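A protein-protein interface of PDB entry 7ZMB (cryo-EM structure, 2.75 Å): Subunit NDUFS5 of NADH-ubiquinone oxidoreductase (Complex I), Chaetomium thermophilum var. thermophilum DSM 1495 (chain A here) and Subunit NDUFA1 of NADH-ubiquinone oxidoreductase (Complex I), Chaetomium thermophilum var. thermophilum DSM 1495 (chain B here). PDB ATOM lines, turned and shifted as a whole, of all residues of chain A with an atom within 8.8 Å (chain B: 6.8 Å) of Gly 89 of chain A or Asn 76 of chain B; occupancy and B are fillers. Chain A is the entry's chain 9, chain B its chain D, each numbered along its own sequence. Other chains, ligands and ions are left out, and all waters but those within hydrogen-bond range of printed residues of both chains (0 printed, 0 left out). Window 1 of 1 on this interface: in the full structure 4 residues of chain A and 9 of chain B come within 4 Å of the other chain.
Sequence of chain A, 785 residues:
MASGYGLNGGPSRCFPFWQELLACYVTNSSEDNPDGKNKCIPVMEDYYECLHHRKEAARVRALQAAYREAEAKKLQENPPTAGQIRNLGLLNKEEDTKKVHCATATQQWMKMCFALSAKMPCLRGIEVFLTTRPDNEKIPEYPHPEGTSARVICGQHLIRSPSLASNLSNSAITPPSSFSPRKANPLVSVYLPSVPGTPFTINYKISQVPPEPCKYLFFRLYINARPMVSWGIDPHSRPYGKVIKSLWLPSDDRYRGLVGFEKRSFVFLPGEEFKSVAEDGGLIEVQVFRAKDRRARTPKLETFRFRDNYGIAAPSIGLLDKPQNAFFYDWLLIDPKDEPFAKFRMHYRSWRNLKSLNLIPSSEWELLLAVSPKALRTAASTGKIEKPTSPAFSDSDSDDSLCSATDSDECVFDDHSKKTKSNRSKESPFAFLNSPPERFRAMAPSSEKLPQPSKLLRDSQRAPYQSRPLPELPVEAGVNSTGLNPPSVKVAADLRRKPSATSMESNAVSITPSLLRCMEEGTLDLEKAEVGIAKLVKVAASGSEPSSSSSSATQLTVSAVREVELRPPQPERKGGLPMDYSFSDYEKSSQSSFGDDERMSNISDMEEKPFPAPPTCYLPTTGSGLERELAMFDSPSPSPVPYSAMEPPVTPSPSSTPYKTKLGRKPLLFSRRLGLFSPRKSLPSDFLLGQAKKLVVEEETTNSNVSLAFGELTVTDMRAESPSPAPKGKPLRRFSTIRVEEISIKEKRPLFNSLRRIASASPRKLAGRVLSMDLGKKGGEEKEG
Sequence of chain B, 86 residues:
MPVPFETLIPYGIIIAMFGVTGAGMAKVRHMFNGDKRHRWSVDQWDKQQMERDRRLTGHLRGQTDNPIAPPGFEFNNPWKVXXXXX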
ATOM      1  N   GLN A  84       1.779  17.189 -29.127  1.00  0.00           N
ATOM      2  CA  GLN A  84       2.057  18.594 -29.505  1.00  0.00           C
ATOM      3  C   GLN A  84       0.866  19.463 -29.103  1.00  0.00           C
ATOM      4  O   GLN A  84       1.096  20.575 -28.598  1.00  0.00           O
ATOM      5  CB  GLN A  84       2.414  18.666 -30.989  1.00  0.00           C
ATOM      6  CG  GLN A  84       3.749  18.004 -31.289  1.00  0.00           C
ATOM      7  CD  GLN A  84       4.000  17.804 -32.761  1.00  0.00           C
ATOM      8  OE1 GLN A  84       3.140  18.057 -33.599  1.00  0.00           O
ATOM      9  NE2 GLN A  84       5.194  17.337 -33.087  1.00  0.00           N
ATOM     10  N   ILE A  85      -0.353  18.969 -29.317  1.00  0.00           N
ATOM     11  CA  ILE A  85      -1.573  19.730 -28.917  1.00  0.00           C
ATOM     12  C   ILE A  85      -1.585  19.866 -27.394  1.00  0.00           C
ATOM     13  O   ILE A  85      -1.930  20.954 -26.903  1.00  0.00           O
ATOM     14  CB  ILE A  85      -2.853  19.067 -29.449  1.00  0.00           C
ATOM     15  CG1 ILE A  85      -2.722  18.691 -30.924  1.00  0.00           C
ATOM     16  CG2 ILE A  85      -4.054  19.968 -29.220  1.00  0.00           C
ATOM     17  CD1 ILE A  85      -2.403  19.859 -31.822  1.00  0.00           C
ATOM     18  N   ARG A  86      -1.198  18.807 -26.685  1.00  0.00           N
ATOM     19  CA  ARG A  86      -1.169  18.812 -25.200  1.00  0.00           C
ATOM     20  C   ARG A  86      -0.120  19.812 -24.703  1.00  0.00           C
ATOM     21  O   ARG A  86      -0.206  20.228 -23.540  1.00  0.00           O
ATOM     22  CB  ARG A  86      -0.857  17.411 -24.665  1.00  0.00           C
ATOM     23  CG  ARG A  86      -2.045  16.649 -24.098  1.00  0.00           C
ATOM     24  CD  ARG A  86      -2.916  16.067 -25.191  1.00  0.00           C
ATOM     25  NE  ARG A  86      -3.845  15.030 -24.769  1.00  0.00           N
ATOM     26  CZ  ARG A  86      -3.654  13.733 -24.975  1.00  0.00           C
ATOM     27  NH1 ARG A  86      -2.568  13.314 -25.601  1.00  0.00           N
ATOM     28  NH2 ARG A  86      -4.553  12.859 -24.562  1.00  0.00           N
ATOM     29  N   ASN A  87       0.844  20.178 -25.541  1.00  0.00           N
ATOM     30  CA  ASN A  87       1.952  21.064 -25.092  1.00  0.00           C
ATOM     31  C   ASN A  87       1.672  22.525 -25.456  1.00  0.00           C
ATOM     32  O   ASN A  87       2.563  23.359 -25.226  1.00  0.00           O
ATOM     33  CB  ASN A  87       3.314  20.576 -25.587  1.00  0.00           C
ATOM     34  CG  ASN A  87       3.738  19.278 -24.937  1.00  0.00           C
ATOM     35  OD1 ASN A  87       3.109  18.821 -23.986  1.00  0.00           O
ATOM     36  ND2 ASN A  87       4.800  18.675 -25.445  1.00  0.00           N
ATOM     37  N   LEU A  88       0.483  22.826 -25.973  1.00  0.00           N
ATOM     38  CA  LEU A  88       0.131  24.203 -26.270  1.00  0.00           C
ATOM     39  C   LEU A  88       0.071  25.041 -25.000  1.00  0.00           C
ATOM     40  O   LEU A  88      -0.565  24.657 -24.015  1.00  0.00           O
ATOM     41  CB  LEU A  88      -1.213  24.250 -26.986  1.00  0.00           C
ATOM     42  CG  LEU A  88      -1.612  25.620 -27.520  1.00  0.00           C
ATOM     43  CD1 LEU A  88      -0.808  25.945 -28.755  1.00  0.00           C
ATOM     44  CD2 LEU A  88      -3.089  25.645 -27.828  1.00  0.00           C
ATOM     45  N   GLY A  89       0.732  26.194 -25.034  1.00  0.00           N
ATOM     46  CA  GLY A  89       0.714  27.122 -23.916  1.00  0.00           C
ATOM     47  C   GLY A  89       1.314  26.588 -22.635  1.00  0.00           C
ATOM     48  O   GLY A  89       0.749  26.796 -21.554  1.00  0.00           O
ATOM     49  N   LEU A  90       2.445  25.902 -22.722  1.00  0.00           N
ATOM     50  CA  LEU A  90       3.122  25.402 -21.540  1.00  0.00           C
ATOM     51  C   LEU A  90       4.270  26.333 -21.160  1.00  0.00           C
ATOM     52  O   LEU A  90       4.490  27.377 -21.776  1.00  0.00           O
ATOM     53  CB  LEU A  90       3.605  23.969 -21.766  1.00  0.00           C
ATOM     54  CG  LEU A  90       2.492  22.921 -21.700  1.00  0.00           C
ATOM     55  CD1 LEU A  90       3.079  21.519 -21.599  1.00  0.00           C
ATOM     56  CD2 LEU A  90       1.537  23.203 -20.546  1.00  0.00           C
ATOM     57  N   LEU A  91       5.015  25.943 -20.125  1.00  0.00           N
ATOM     58  CA  LEU A  91       6.033  26.832 -19.576  1.00  0.00           C
ATOM     59  C   LEU A  91       7.337  26.769 -20.361  1.00  0.00           C
ATOM     60  O   LEU A  91       7.979  27.802 -20.580  1.00  0.00           O
ATOM     61  CB  LEU A  91       6.286  26.496 -18.106  1.00  0.00           C
ATOM     62  CG  LEU A  91       7.276  27.407 -17.377  1.00  0.00           C
ATOM     63  CD1 LEU A  91       6.758  28.835 -17.336  1.00  0.00           C
ATOM     64  CD2 LEU A  91       7.547  26.892 -15.972  1.00  0.00           C
ATOM     65  N   ASN A  92       7.750  25.576 -20.791  1.00  0.00           N
ATOM     66  CA  ASN A  92       9.045  25.427 -21.441  1.00  0.00           C
ATOM     67  C   ASN A  92       8.945  24.599 -22.714  1.00  0.00           C
ATOM     68  O   ASN A  92       9.871  23.849 -23.044  1.00  0.00           O
ATOM     69  CB  ASN A  92      10.063  24.797 -20.489  1.00  0.00           C
ATOM     70  CG  ASN A  92      11.470  25.302 -20.727  1.00  0.00           C
ATOM     71  OD1 ASN A  92      11.705  26.125 -21.610  1.00  0.00           O
ATOM     72  ND2 ASN A  92      12.416  24.810 -19.935  1.00  0.00           N
ATOM     73  N   LYS A  93       7.843  24.724 -23.445  1.00  0.00           N
ATOM     74  CA  LYS A  93       7.607  23.970 -24.673  1.00  0.00           C
ATOM     75  C   LYS A  93       7.284  24.920 -25.818  1.00  0.00           C
ATOM     76  O   LYS A  93       6.319  24.734 -26.563  1.00  0.00           O
ATOM     77  CB  LYS A  93       6.490  22.948 -24.482  1.00  0.00           C
ATOM     78  CG  LYS A  93       6.632  22.092 -23.234  1.00  0.00           C
ATOM     79  CD  LYS A  93       7.928  21.297 -23.244  1.00  0.00           C
ATOM     80  CE  LYS A  93       7.825  20.068 -24.129  1.00  0.00           C
ATOM     81  NZ  LYS A  93       9.038  19.210 -24.025  1.00  0.00           N
ATOM     82  N   GLU A  94       8.104  25.964 -25.967  1.00  0.00           N
ATOM     83  CA  GLU A  94       7.861  26.966 -27.000  1.00  0.00           C
ATOM     84  C   GLU A  94       7.881  26.358 -28.396  1.00  0.00           C
ATOM     85  O   GLU A  94       7.093  26.765 -29.258  1.00  0.00           O
ATOM     86  CB  GLU A  94       8.897  28.085 -26.904  1.00  0.00           C
ATOM     87  CG  GLU A  94       8.618  29.103 -25.815  1.00  0.00           C
ATOM     88  CD  GLU A  94       9.348  28.788 -24.525  1.00  0.00           C
ATOM     89  OE1 GLU A  94       9.812  27.638 -24.370  1.00  0.00           O
ATOM     90  OE2 GLU A  94       9.462  29.688 -23.668  1.00  0.00           O
ATOM     91  N   ASP A  96       6.958  23.365 -29.415  1.00  0.00           N
ATOM     92  CA  ASP A  96       5.731  22.639 -29.724  1.00  0.00           C
ATOM     93  C   ASP A  96       4.586  23.586 -30.051  1.00  0.00           C
ATOM     94  O   ASP A  96       3.820  23.338 -30.988  1.00  0.00           O
ATOM     95  CB  ASP A  96       5.357  21.725 -28.559  1.00  0.00           C
ATOM     96  CG  ASP A  96       6.011  20.364 -28.656  1.00  0.00           C
ATOM     97  OD1 ASP A  96       6.239  19.893 -29.789  1.00  0.00           O
ATOM     98  OD2 ASP A  96       6.298  19.763 -27.598  1.00  0.00           O
ATOM     99  N   THR A  97       4.446  24.671 -29.286  1.00  0.00           N
ATOM    100  CA  THR A  97       3.357  25.612 -29.527  1.00  0.00           C
ATOM    101  C   THR A  97       3.484  26.274 -30.890  1.00  0.00           C
ATOM    102  O   THR A  97       2.486  26.441 -31.601  1.00  0.00           O
ATOM    103  CB  THR A  97       3.313  26.660 -28.416  1.00  0.00           C
ATOM    104  OG1 THR A  97       2.953  26.032 -27.180  1.00  0.00           O
ATOM    105  CG2 THR A  97       2.310  27.758 -28.734  1.00  0.00           C
ATOM    106  N   LYS A  98       4.704  26.650 -31.278  1.00  0.00           N
ATOM    107  CA  LYS A  98       4.901  27.293 -32.574  1.00  0.00           C
ATOM    108  C   LYS A  98       4.507  26.361 -33.711  1.00  0.00           C
ATOM    109  O   LYS A  98       3.901  26.791 -34.701  1.00  0.00           O
ATOM    110  CB  LYS A  98       6.353  27.746 -32.721  1.00  0.00           C
ATOM    111  CG  LYS A  98       6.775  28.805 -31.717  1.00  0.00           C
ATOM    112  CD  LYS A  98       8.099  29.438 -32.107  1.00  0.00           C
ATOM    113  CE  LYS A  98       7.961  30.271 -33.369  1.00  0.00           C
ATOM    114  NZ  LYS A  98       7.025  31.413 -33.175  1.00  0.00           N
ATOM    115  N   VAL A 100       2.260  23.973 -33.520  1.00  0.00           N
ATOM    116  CA  VAL A 100       0.806  23.827 -33.496  1.00  0.00           C
ATOM    117  C   VAL A 100       0.131  25.028 -34.142  1.00  0.00           C
ATOM    118  O   VAL A 100      -0.799  24.879 -34.945  1.00  0.00           O
ATOM    119  CB  VAL A 100       0.315  23.611 -32.054  1.00  0.00           C
ATOM    120  CG1 VAL A 100      -1.199  23.660 -32.001  1.00  0.00           C
ATOM    121  CG2 VAL A 100       0.819  22.284 -31.521  1.00  0.00           C
ATOM    122  N   HIS A 101       0.583  26.233 -33.814  1.00  0.00           N
ATOM    123  CA  HIS A 101      -0.029  27.432 -34.367  1.00  0.00           C
ATOM    124  C   HIS A 101       0.526  27.817 -35.731  1.00  0.00           C
ATOM    125  O   HIS A 101       0.026  28.774 -36.332  1.00  0.00           O
ATOM    126  CB  HIS A 101       0.142  28.603 -33.399  1.00  0.00           C
ATOM    127  CG  HIS A 101      -0.784  28.549 -32.228  1.00  0.00           C
ATOM    128  ND1 HIS A 101      -1.977  27.863 -32.259  1.00  0.00           N
ATOM    129  CD2 HIS A 101      -0.698  29.101 -30.996  1.00  0.00           C
ATOM    130  CE1 HIS A 101      -2.585  27.990 -31.093  1.00  0.00           C
ATOM    131  NE2 HIS A 101      -1.831  28.738 -30.309  1.00  0.00           N
ATOM    132  N   ARG B  54      -3.782  22.617 -15.448  1.00  0.00           N
ATOM    133  CA  ARG B  54      -3.249  21.826 -16.586  1.00  0.00           C
ATOM    134  C   ARG B  54      -2.946  22.771 -17.747  1.00  0.00           C
ATOM    135  O   ARG B  54      -1.934  22.560 -18.414  1.00  0.00           O
ATOM    136  CB  ARG B  54      -4.258  20.748 -16.970  1.00  0.00           C
ATOM    137  CG  ARG B  54      -3.686  19.629 -17.823  1.00  0.00           C
ATOM    138  CD  ARG B  54      -4.781  18.943 -18.610  1.00  0.00           C
ATOM    139  NE  ARG B  54      -5.387  17.808 -17.936  1.00  0.00           N
ATOM    140  CZ  ARG B  54      -6.549  17.276 -18.284  1.00  0.00           C
ATOM    141  NH1 ARG B  54      -7.023  16.229 -17.634  1.00  0.00           N
ATOM    142  NH2 ARG B  54      -7.239  17.804 -19.278  1.00  0.00           N
ATOM    143  N   ARG B  55      -3.787  23.780 -17.966  1.00  0.00           N
ATOM    144  CA  ARG B  55      -3.566  24.764 -19.049  1.00  0.00           C
ATOM    145  C   ARG B  55      -2.251  25.530 -18.850  1.00  0.00           C
ATOM    146  O   ARG B  55      -1.666  25.936 -19.860  1.00  0.00           O
ATOM    147  CB  ARG B  55      -4.772  25.691 -19.189  1.00  0.00           C
ATOM    148  CG  ARG B  55      -6.025  25.027 -19.735  1.00  0.00           C
ATOM    149  CD  ARG B  55      -7.128  26.055 -19.654  1.00  0.00           C
ATOM    150  NE  ARG B  55      -6.799  27.211 -20.468  1.00  0.00           N
ATOM    151  CZ  ARG B  55      -7.405  28.384 -20.382  1.00  0.00           C
ATOM    152  NH1 ARG B  55      -8.374  28.563 -19.504  1.00  0.00           N
ATOM    153  NH2 ARG B  55      -7.037  29.374 -21.173  1.00  0.00           N
ATOM    154  N   LEU B  56      -1.814  25.720 -17.605  1.00  0.00           N
ATOM    155  CA  LEU B  56      -0.567  26.475 -17.322  1.00  0.00           C
ATOM    156  C   LEU B  56       0.617  25.548 -17.011  1.00  0.00           C
ATOM    157  O   LEU B  56       1.745  26.015 -17.152  1.00  0.00           O
ATOM    158  CB  LEU B  56      -0.835  27.422 -16.151  1.00  0.00           C
ATOM    159  CG  LEU B  56      -1.882  28.509 -16.371  1.00  0.00           C
ATOM    160  CD1 LEU B  56      -2.656  28.794 -15.095  1.00  0.00           C
ATOM    161  CD2 LEU B  56      -1.235  29.779 -16.886  1.00  0.00           C
ATOM    162  N   THR B  57       0.383  24.301 -16.579  1.00  0.00           N
ATOM    163  CA  THR B  57       1.497  23.461 -16.162  1.00  0.00           C
ATOM    164  C   THR B  57       1.506  22.071 -16.771  1.00  0.00           C
ATOM    165  O   THR B  57       2.516  21.376 -16.633  1.00  0.00           O
ATOM    166  CB  THR B  57       1.525  23.309 -14.631  1.00  0.00           C
ATOM    167  OG1 THR B  57       0.481  22.424 -14.215  1.00  0.00           O
ATOM    168  CG2 THR B  57       1.353  24.643 -13.939  1.00  0.00           C
ATOM    169  N   GLY B  58       0.434  21.640 -17.429  1.00  0.00           N
ATOM    170  CA  GLY B  58       0.335  20.303 -17.964  1.00  0.00           C
ATOM    171  C   GLY B  58      -0.136  19.272 -16.961  1.00  0.00           C
ATOM    172  O   GLY B  58      -0.694  18.246 -17.348  1.00  0.00           O
ATOM    173  N   ALA B  69       0.791  34.883 -18.450  1.00  0.00           N
ATOM    174  CA  ALA B  69       0.447  33.548 -18.981  1.00  0.00           C
ATOM    175  C   ALA B  69       1.491  33.066 -19.984  1.00  0.00           C
ATOM    176  O   ALA B  69       2.044  33.902 -20.714  1.00  0.00           O
ATOM    177  CB  ALA B  69      -0.957  33.523 -19.552  1.00  0.00           C
ATOM    178  N   PRO B  70       1.759  31.746 -20.057  1.00  0.00           N
ATOM    179  CA  PRO B  70       2.638  31.208 -21.078  1.00  0.00           C
ATOM    180  C   PRO B  70       1.973  31.489 -22.431  1.00  0.00           C
ATOM    181  O   PRO B  70       0.771  31.476 -22.514  1.00  0.00           O
ATOM    182  CB  PRO B  70       2.626  29.712 -20.761  1.00  0.00           C
ATOM    183  CG  PRO B  70       1.374  29.482 -19.961  1.00  0.00           C
ATOM    184  CD  PRO B  70       1.240  30.741 -19.145  1.00  0.00           C
ATOM    185  N   PRO B  71       2.723  31.807 -23.498  1.00  0.00           N
ATOM    186  CA  PRO B  71       2.111  32.143 -24.781  1.00  0.00           C
ATOM    187  C   PRO B  71       1.359  30.924 -25.332  1.00  0.00           C
ATOM    188  O   PRO B  71       1.868  29.840 -25.217  1.00  0.00           O
ATOM    189  CB  PRO B  71       3.300  32.545 -25.662  1.00  0.00           C
ATOM    190  CG  PRO B  71       4.503  31.901 -25.005  1.00  0.00           C
ATOM    191  CD  PRO B  71       4.184  31.878 -23.525  1.00  0.00           C
ATOM    192  N   GLY B  72       0.187  31.136 -25.937  1.00  0.00           N
ATOM    193  CA  GLY B  72      -0.641  30.015 -26.427  1.00  0.00           C
ATOM    194  C   GLY B  72      -1.647  29.582 -25.388  1.00  0.00           C
ATOM    195  O   GLY B  72      -2.390  28.634 -25.671  1.00  0.00           O
ATOM    196  N   PHE B  73      -1.685  30.263 -24.245  1.00  0.00           N
ATOM    197  CA  PHE B  73      -2.649  29.939 -23.163  1.00  0.00           C
ATOM    198  C   PHE B  73      -4.021  30.441 -23.606  1.00  0.00           C
ATOM    199  O   PHE B  73      -5.045  29.857 -23.209  1.00  0.00           O
ATOM    200  CB  PHE B  73      -2.163  30.531 -21.841  1.00  0.00           C
ATOM    201  CG  PHE B  73      -3.117  30.414 -20.684  1.00  0.00           C
ATOM    202  CD1 PHE B  73      -3.241  29.227 -19.981  1.00  0.00           C
ATOM    203  CD2 PHE B  73      -3.877  31.502 -20.284  1.00  0.00           C
ATOM    204  CE1 PHE B  73      -4.115  29.127 -18.913  1.00  0.00           C
ATOM    205  CE2 PHE B  73      -4.744  31.399 -19.211  1.00  0.00           C
ATOM    206  CZ  PHE B  73      -4.863  30.213 -18.528  1.00  0.00           C
ATOM    207  N   GLU B  74      -4.027  31.450 -24.473  1.00  0.00           N
ATOM    208  CA  GLU B  74      -5.288  32.024 -24.982  1.00  0.00           C
ATOM    209  C   GLU B  74      -5.947  31.023 -25.945  1.00  0.00           C
ATOM    210  O   GLU B  74      -7.091  31.262 -26.336  1.00  0.00           O
ATOM    211  CB  GLU B  74      -4.947  33.362 -25.625  1.00  0.00           C
ATOM    212  CG  GLU B  74      -3.548  33.403 -26.206  1.00  0.00           C
ATOM    213  CD  GLU B  74      -3.120  34.764 -26.721  1.00  0.00           C
ATOM    214  OE1 GLU B  74      -1.904  34.980 -26.868  1.00  0.00           O
ATOM    215  OE2 GLU B  74      -4.007  35.606 -26.973  1.00  0.00           O
ATOM    216  N   PHE B  75      -5.240  29.950 -26.311  1.00  0.00           N
ATOM    217  CA  PHE B  75      -5.752  28.973 -27.303  1.00  0.00           C
ATOM    218  C   PHE B  75      -5.964  27.575 -26.720  1.00  0.00           C
ATOM    219  O   PHE B  75      -6.735  26.842 -27.334  1.00  0.00           O
ATOM    220  CB  PHE B  75      -4.762  28.894 -28.463  1.00  0.00           C
ATOM    221  CG  PHE B  75      -4.510  30.209 -29.154  1.00  0.00           C
ATOM    222  CD1 PHE B  75      -3.390  30.966 -28.860  1.00  0.00           C
ATOM    223  CD2 PHE B  75      -5.396  30.690 -30.102  1.00  0.00           C
ATOM    224  CE1 PHE B  75      -3.154  32.166 -29.509  1.00  0.00           C
ATOM    225  CE2 PHE B  75      -5.163  31.895 -30.743  1.00  0.00           C
ATOM    226  CZ  PHE B  75      -4.043  32.629 -30.449  1.00  0.00           C
ATOM    227  N   ASN B  76      -5.338  27.204 -25.604  1.00  0.00           N
ATOM    228  CA  ASN B  76      -5.485  25.834 -25.128  1.00  0.00           C
ATOM    229  C   ASN B  76      -6.711  25.631 -24.259  1.00  0.00           C
ATOM    230  O   ASN B  76      -6.874  24.543 -23.704  1.00  0.00           O
ATOM    231  CB  ASN B  76      -4.236  25.398 -24.353  1.00  0.00           C
ATOM    232  CG  ASN B  76      -3.846  26.376 -23.258  1.00  0.00           C
ATOM    233  OD1 ASN B  76      -4.694  27.022 -22.654  1.00  0.00           O
ATOM    234  ND2 ASN B  76      -2.553  26.485 -23.000  1.00  0.00           N
ATOM    235  N   ASN B  77      -7.560  26.656 -24.109  1.00  0.00           N
ATOM    236  CA  ASN B  77      -8.766  26.534 -23.239  1.00  0.00           C
ATOM    237  C   ASN B  77      -9.584  25.369 -23.773  1.00  0.00           C
ATOM    238  O   ASN B  77     -10.064  25.466 -24.907  1.00  0.00           O
ATOM    239  CB  ASN B  77      -9.588  27.820 -23.155  1.00  0.00           C
ATOM    240  CG  ASN B  77     -10.639  27.797 -22.068  1.00  0.00           C
ATOM    241  OD1 ASN B  77     -10.532  27.045 -21.103  1.00  0.00           O
ATOM    242  ND2 ASN B  77     -11.656  28.634 -22.204  1.00  0.00           N
ATOM    243  N   PRO B  78      -9.775  24.273 -23.016  1.00  0.00           N
ATOM    244  CA  PRO B  78     -10.441  23.103 -23.573  1.00  0.00           C
ATOM    245  C   PRO B  78     -11.954  23.254 -23.765  1.00  0.00           C
ATOM    246  O   PRO B  78     -12.586  23.769 -22.881  1.00  0.00           O
ATOM    247  CB  PRO B  78     -10.136  22.034 -22.514  1.00  0.00           C
ATOM    248  CG  PRO B  78     -10.047  22.811 -21.224  1.00  0.00           C
ATOM    249  CD  PRO B  78      -9.375  24.107 -21.618  1.00  0.00           C
ATOM    250  N   TRP B  79     -12.476  22.855 -24.921  1.00  0.00           N
ATOM    251  CA  TRP B  79     -13.950  22.821 -25.101  1.00  0.00           C
ATOM    252  C   TRP B  79     -14.306  21.338 -25.157  1.00  0.00           C
ATOM    253  O   TRP B  79     -13.732  20.644 -25.995  1.00  0.00           O
ATOM    254  CB  TRP B  79     -14.411  23.626 -26.314  1.00  0.00           C
ATOM    255  CG  TRP B  79     -14.703  25.064 -26.014  1.00  0.00           C
ATOM    256  CD1 TRP B  79     -14.268  25.789 -24.945  1.00  0.00           C
ATOM    257  CD2 TRP B  79     -15.496  25.963 -26.809  1.00  0.00           C
ATOM    258  NE1 TRP B  79     -14.738  27.071 -25.013  1.00  0.00           N
ATOM    259  CE2 TRP B  79     -15.494  27.208 -26.147  1.00  0.00           C
ATOM    260  CE3 TRP B  79     -16.204  25.838 -28.008  1.00  0.00           C
ATOM    261  CZ2 TRP B  79     -16.172  28.317 -26.648  1.00  0.00           C
ATOM    262  CZ3 TRP B  79     -16.877  26.934 -28.501  1.00  0.00           C
ATOM    263  CH2 TRP B  79     -16.858  28.156 -27.829  1.00  0.00           C
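ND2 of Asn 76 of chain B is in hydrogen-bond range of O of Leu 88 of chain A, at 2.9 Å.
The backbone carbonyl oxygen (O) of Gly 89 of chain A sits close to the backbone carbonyl oxygen (O) of Arg 55 of chain B, 3.1 Å away.
O of Phe 73 of chain B is in hydrogen-bond range of NH2 of Arg 55 of chain B (2.9 Å).
The side-chain amide oxygen of Asn 76 of chain B lies within hydrogen-bond range of the guanidinium group of Arg 55 of chain B (3.0 Å).
The guanidinium group (NH1) of Arg 55 of chain B lies within hydrogen-bond range of the side-chain amide oxygen (OD1) of Asn 77 of chain B, 3.1 Å away.
The backbone carbonyl oxygen (O) of Gly 72 of chain B lies within hydrogen-bond range of the side-chain amide nitrogen (ND2) of Asn 76 of chain B, 3.4 Å away.
OD1 of Asn 76 of chain B lies close to O of Phe 73 of chain B (2.9 Å).
N of Gly 89 of chain A sits at hydrogen-bond distance from OG1 of Thr 97 of chain A.
Among the printed residues, merely in contact across the chains: His 101 of chain A with Phe 75 of chain B (3.1 Å), Leu 90 of chain A with Pro 70 of chain B (3.2 Å), Gly 89 of chain A with Pro 70 of chain B (3.2 Å), Gly 89 of chain A with Pro 71 of chain B (3.2 Å), Gly 89 of chain A with Asn 76 of chain B (3.5 Å), Leu 88 of chain A with Gly 72 of chain B (3.6 Å), Leu 88 of chain A with Phe 75 of chain B (3.6 Å), Leu 90 of chain A with Gly 58 of chain B (3.7 Å), Gly 89 of chain A with Gly 72 of chain B (3.7 Å), Leu 90 of chain A with Thr 57 of chain B (3.9 Å) and Gly 89 of chain A with Phe 73 of chain B (3.97 Å).
Of chain B, only Arg 55 (3.1 Å), Pro 70 (3.2 Å), Pro 71 (3.2 Å), Gly 72 (3.7 Å), Phe 73 (3.97 Å) and Asn 76 (3.5 Å) come within 4 Å of Gly 89 of chain A.
Gly 72 of chain B touches two residues of chain A.
Of the printed residues of chain B, Leu 90 of chain A touches Thr 57 (3.9 Å), Gly 58 (3.7 Å) and Pro 70 (3.2 Å).
Of the printed residues of chain A, Phe 73 of chain B touches Gly 89 (3.97 Å).
Printed residues of chain A within 4 Å of Arg 55 of chain B: Gly 89 (3.1 Å).
The nearest residue of chain B that does not touch Gly 89 of chain A is Leu 56 of chain B (4.4 Å).
Of the 16 printed residues of chain A, 4 touch a printed residue of chain B.
Hydrophobic or aromatic side chains of chain A within 4 Å of the printed part of chain B: Leu 88, Leu 90 and His 101.
Printed residues of chain B that touch a printed residue of chain A: Arg 55, Thr 57, Gly 58, Pro 70, Pro 71, Gly 72, Phe 73, Phe 75 and Asn 76.
Hydrophobic or aromatic side chains of chain B within 4 Å of the printed part of chain A: Pro 70 and Phe 75.
Among the printed residues, no Asp or Glu carboxylate lies within 4 Å of a Lys or Arg side-chain nitrogen of the other chain.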
